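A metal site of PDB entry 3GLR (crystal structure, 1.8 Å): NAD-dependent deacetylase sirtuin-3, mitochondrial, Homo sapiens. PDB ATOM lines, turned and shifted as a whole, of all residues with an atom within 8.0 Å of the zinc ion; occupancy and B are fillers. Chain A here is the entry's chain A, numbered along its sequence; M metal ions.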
ATOM      1  N   THR A 141      20.882  -5.254  -9.744  1.00  0.00           N
ATOM      2  CA  THR A 141      20.754  -4.802  -8.339  1.00  0.00           C
ATOM      3  C   THR A 141      20.460  -3.294  -8.346  1.00  0.00           C
ATOM      4  O   THR A 141      21.134  -2.524  -9.022  1.00  0.00           O
ATOM      5  CB  THR A 141      22.068  -5.066  -7.546  1.00  0.00           C
ATOM      6  OG1 THR A 141      22.333  -6.476  -7.528  1.00  0.00           O
ATOM      7  CG2 THR A 141      21.958  -4.571  -6.085  1.00  0.00           C
ATOM      8  N   CYS A 142      19.439  -2.877  -7.606  1.00  0.00           N
ATOM      9  CA  CYS A 142      19.235  -1.407  -7.439  1.00  0.00           C
ATOM     10  C   CYS A 142      20.472  -0.761  -6.797  1.00  0.00           C
ATOM     11  O   CYS A 142      20.937  -1.196  -5.731  1.00  0.00           O
ATOM     12  CB  CYS A 142      18.013  -1.111  -6.574  1.00  0.00           C
ATOM     13  SG  CYS A 142      17.736   0.701  -6.513  1.00  0.00           S
ATOM     14  N   THR A 143      21.013   0.274  -7.445  1.00  0.00           N
ATOM     15  CA  THR A 143      22.187   0.977  -6.909  1.00  0.00           C
ATOM     16  C   THR A 143      21.915   1.741  -5.618  1.00  0.00           C
ATOM     17  O   THR A 143      22.846   2.088  -4.907  1.00  0.00           O
ATOM     18  CB  THR A 143      22.771   1.957  -7.917  1.00  0.00           C
ATOM     19  OG1 THR A 143      21.757   2.912  -8.290  1.00  0.00           O
ATOM     20  CG2 THR A 143      23.285   1.179  -9.152  1.00  0.00           C
ATOM     21  N   VAL A 144      20.637   1.988  -5.326  1.00  0.00           N
ATOM     22  CA  VAL A 144      20.286   2.729  -4.100  1.00  0.00           C
ATOM     23  C   VAL A 144      19.799   1.795  -2.992  1.00  0.00           C
ATOM     24  O   VAL A 144      20.374   1.776  -1.911  1.00  0.00           O
ATOM     25  CB  VAL A 144      19.223   3.800  -4.381  1.00  0.00           C
ATOM     26  CG1 VAL A 144      18.764   4.518  -3.043  1.00  0.00           C
ATOM     27  CG2 VAL A 144      19.762   4.806  -5.452  1.00  0.00           C
ATOM     28  N   CYS A 145      18.759   1.012  -3.250  1.00  0.00           N
ATOM     29  CA  CYS A 145      18.201   0.214  -2.169  1.00  0.00           C
ATOM     30  C   CYS A 145      18.731  -1.218  -2.103  1.00  0.00           C
ATOM     31  O   CYS A 145      18.365  -1.965  -1.191  1.00  0.00           O
ATOM     32  CB  CYS A 145      16.668   0.197  -2.230  1.00  0.00           C
ATOM     33  SG  CYS A 145      15.960  -0.854  -3.525  1.00  0.00           S
ATOM     34  N   GLN A 146      19.513  -1.633  -3.107  1.00  0.00           N
ATOM     35  CA  GLN A 146      20.095  -2.971  -3.158  1.00  0.00           C
ATOM     36  C   GLN A 146      19.129  -4.126  -3.430  1.00  0.00           C
ATOM     37  O   GLN A 146      19.520  -5.285  -3.291  1.00  0.00           O
ATOM     38  CB  GLN A 146      20.919  -3.250  -1.882  1.00  0.00           C
ATOM     39  CG  GLN A 146      21.962  -2.189  -1.572  1.00  0.00           C
ATOM     40  CD  GLN A 146      22.831  -1.828  -2.745  1.00  0.00           C
ATOM     41  OE1 GLN A 146      23.338  -2.683  -3.456  1.00  0.00           O
ATOM     42  NE2 GLN A 146      23.024  -0.541  -2.942  1.00  0.00           N
ATOM     43  N   ARG A 147      17.877  -3.852  -3.790  1.00  0.00           N
ATOM     44  CA  ARG A 147      16.966  -4.928  -4.212  1.00  0.00           C
ATOM     45  C   ARG A 147      17.506  -5.663  -5.424  1.00  0.00           C
ATOM     46  O   ARG A 147      17.933  -5.014  -6.399  1.00  0.00           O
ATOM     47  CB  ARG A 147      15.601  -4.328  -4.578  1.00  0.00           C
ATOM     48  CG  ARG A 147      14.674  -4.189  -3.378  1.00  0.00           C
ATOM     49  CD  ARG A 147      13.231  -3.889  -3.783  1.00  0.00           C
ATOM     50  NE  ARG A 147      12.335  -3.847  -2.617  1.00  0.00           N
ATOM     51  CZ  ARG A 147      12.409  -2.916  -1.667  1.00  0.00           C
ATOM     52  NH1 ARG A 147      11.558  -2.918  -0.636  1.00  0.00           N
ATOM     53  NH2 ARG A 147      13.338  -1.969  -1.748  1.00  0.00           N
ATOM     54  N   PRO A 148      17.517  -7.014  -5.404  1.00  0.00           N
ATOM     55  CA  PRO A 148      17.951  -7.770  -6.577  1.00  0.00           C
ATOM     56  C   PRO A 148      16.787  -7.984  -7.548  1.00  0.00           C
ATOM     57  O   PRO A 148      15.620  -8.054  -7.127  1.00  0.00           O
ATOM     58  CB  PRO A 148      18.371  -9.126  -5.977  1.00  0.00           C
ATOM     59  CG  PRO A 148      17.425  -9.282  -4.850  1.00  0.00           C
ATOM     60  CD  PRO A 148      17.295  -7.910  -4.245  1.00  0.00           C
ATOM     61  N   PHE A 149      17.096  -8.069  -8.825  1.00  0.00           N
ATOM     62  CA  PHE A 149      16.121  -8.363  -9.867  1.00  0.00           C
ATOM     63  C   PHE A 149      16.712  -9.365 -10.841  1.00  0.00           C
ATOM     64  O   PHE A 149      17.896  -9.268 -11.166  1.00  0.00           O
ATOM     65  CB  PHE A 149      15.760  -7.090 -10.647  1.00  0.00           C
ATOM     66  CG  PHE A 149      15.216  -5.993  -9.782  1.00  0.00           C
ATOM     67  CD1 PHE A 149      13.852  -5.918  -9.496  1.00  0.00           C
ATOM     68  CD2 PHE A 149      16.062  -5.029  -9.249  1.00  0.00           C
ATOM     69  CE1 PHE A 149      13.334  -4.895  -8.661  1.00  0.00           C
ATOM     70  CE2 PHE A 149      15.576  -3.985  -8.444  1.00  0.00           C
ATOM     71  CZ  PHE A 149      14.212  -3.910  -8.158  1.00  0.00           C
ATOM     72  N   ARG A 165      14.918   1.865 -14.014  1.00  0.00           N
ATOM     73  CA  ARG A 165      14.746   2.455 -12.704  1.00  0.00           C
ATOM     74  C   ARG A 165      14.084   1.451 -11.762  1.00  0.00           C
ATOM     75  O   ARG A 165      13.328   0.587 -12.198  1.00  0.00           O
ATOM     76  CB  ARG A 165      13.905   3.727 -12.795  1.00  0.00           C
ATOM     77  CG  ARG A 165      14.600   4.878 -13.489  1.00  0.00           C
ATOM     78  CD  ARG A 165      15.461   5.674 -12.523  1.00  0.00           C
ATOM     79  NE  ARG A 165      16.449   6.492 -13.215  1.00  0.00           N
ATOM     80  CZ  ARG A 165      17.315   7.304 -12.600  1.00  0.00           C
ATOM     81  NH1 ARG A 165      17.306   7.402 -11.280  1.00  0.00           N
ATOM     82  NH2 ARG A 165      18.184   8.014 -13.310  1.00  0.00           N
ATOM     83  N   CYS A 166      14.372   1.582 -10.480  1.00  0.00           N
ATOM     84  CA  CYS A 166      13.837   0.675  -9.475  1.00  0.00           C
ATOM     85  C   CYS A 166      12.361   0.982  -9.227  1.00  0.00           C
ATOM     86  O   CYS A 166      11.998   2.157  -8.997  1.00  0.00           O
ATOM     87  CB  CYS A 166      14.597   0.861  -8.169  1.00  0.00           C
ATOM     88  SG  CYS A 166      14.068  -0.171  -6.784  1.00  0.00           S
ATOM     89  N   PRO A 167      11.508  -0.059  -9.236  1.00  0.00           N
ATOM     90  CA  PRO A 167      10.081   0.173  -9.013  1.00  0.00           C
ATOM     91  C   PRO A 167       9.766   0.541  -7.567  1.00  0.00           C
ATOM     92  O   PRO A 167       8.666   1.036  -7.278  1.00  0.00           O
ATOM     93  CB  PRO A 167       9.450  -1.165  -9.420  1.00  0.00           C
ATOM     94  CG  PRO A 167      10.556  -2.219  -9.161  1.00  0.00           C
ATOM     95  CD  PRO A 167      11.842  -1.492  -9.502  1.00  0.00           C
ATOM     96  N   VAL A 168      10.713   0.337  -6.654  1.00  0.00           N
ATOM     97  CA  VAL A 168      10.461   0.688  -5.271  1.00  0.00           C
ATOM     98  C   VAL A 168      11.016   2.067  -4.891  1.00  0.00           C
ATOM     99  O   VAL A 168      10.293   2.863  -4.291  1.00  0.00           O
ATOM    100  CB  VAL A 168      10.965  -0.403  -4.281  1.00  0.00           C
ATOM    101  CG1 VAL A 168      10.735   0.035  -2.849  1.00  0.00           C
ATOM    102  CG2 VAL A 168      10.195  -1.703  -4.545  1.00  0.00           C
ATOM    103  N   CYS A 169      12.264   2.376  -5.258  1.00  0.00           N
ATOM    104  CA  CYS A 169      12.878   3.642  -4.815  1.00  0.00           C
ATOM    105  C   CYS A 169      13.289   4.618  -5.949  1.00  0.00           C
ATOM    106  O   CYS A 169      13.770   5.705  -5.670  1.00  0.00           O
ATOM    107  CB  CYS A 169      14.104   3.381  -3.948  1.00  0.00           C
ATOM    108  SG  CYS A 169      15.589   2.876  -4.870  1.00  0.00           S
ATOM    109  N   THR A 170      13.065   4.204  -7.194  1.00  0.00           N
ATOM    110  CA  THR A 170      13.492   4.898  -8.453  1.00  0.00           C
ATOM    111  C   THR A 170      14.975   4.985  -8.707  1.00  0.00           C
ATOM    112  O   THR A 170      15.384   5.602  -9.662  1.00  0.00           O
ATOM    113  CB  THR A 170      12.855   6.325  -8.623  1.00  0.00           C
ATOM    114  OG1 THR A 170      13.563   7.251  -7.782  1.00  0.00           O
ATOM    115  CG2 THR A 170      11.387   6.311  -8.272  1.00  0.00           C
ATOM    116  N   GLY A 171      15.815   4.330  -7.914  1.00  0.00           N
ATOM    117  CA  GLY A 171      17.253   4.388  -8.195  1.00  0.00           C
ATOM    118  C   GLY A 171      17.585   3.658  -9.511  1.00  0.00           C
ATOM    119  O   GLY A 171      16.770   2.884 -10.032  1.00  0.00           O
ATOM    120  N   VAL A 172      18.754   3.943 -10.071  1.00  0.00           N
ATOM    121  CA  VAL A 172      19.196   3.224 -11.295  1.00  0.00           C
ATOM    122  C   VAL A 172      19.429   1.770 -10.941  1.00  0.00           C
ATOM    123  O   VAL A 172      20.072   1.481  -9.948  1.00  0.00           O
ATOM    124  CB  VAL A 172      20.503   3.806 -11.846  1.00  0.00           C
ATOM    125  CG1 VAL A 172      21.095   2.886 -12.972  1.00  0.00           C
ATOM    126  CG2 VAL A 172      20.239   5.220 -12.367  1.00  0.00           C
ATOM    127  N   VAL A 173      18.883   0.857 -11.753  1.00  0.00           N
ATOM    128  CA  VAL A 173      19.094  -0.600 -11.490  1.00  0.00           C
ATOM    129  C   VAL A 173      20.230  -1.037 -12.417  1.00  0.00           C
ATOM    130  O   VAL A 173      20.119  -0.856 -13.639  1.00  0.00           O
ATOM    131  CB  VAL A 173      17.842  -1.402 -11.775  1.00  0.00           C
ATOM    132  CG1 VAL A 173      18.125  -2.993 -11.685  1.00  0.00           C
ATOM    133  CG2 VAL A 173      16.732  -1.013 -10.819  1.00  0.00           C
HETATM  134 ZN    ZN M   1      15.695   0.605  -5.325  1.00  0.00          ZN
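The zinc ion is bound by SG of Cys 166 (2.3 Å).
The zinc ion is bound by SG of Cys 169, 2.3 Å away.
The zinc ion is bound by the side-chain sulfur (SG) of Cys 145 (2.3 Å).
The zinc ion is bound by SG of Cys 142, at 2.4 Å.
N of Cys 166 is in hydrogen-bond range of O of Gly 171, at 2.8 Å.
SG of Cys 166 lies close to N of Val 168, 3.4 Å away.
The side-chain sulfur (SG) of Cys 169 lies close to the backbone NH (N) of Gly 171 (3.4 Å).
SG of Cys 145 sits close to NH2 of Arg 147 (3.4 Å).
SG of Cys 142 sits close to N of Val 144, 3.4 Å away.
The backbone NH of Cys 142 lies within hydrogen-bond range of the backbone carbonyl oxygen of Arg 147 (2.9 Å).
Four residues have an atom within 4 Å of the zinc ion: Cys 142, Cys 145, Cys 166 and Cys 169.
The nearest printed residue that does not touch the zinc ion is Gly 171 (4.5 Å).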
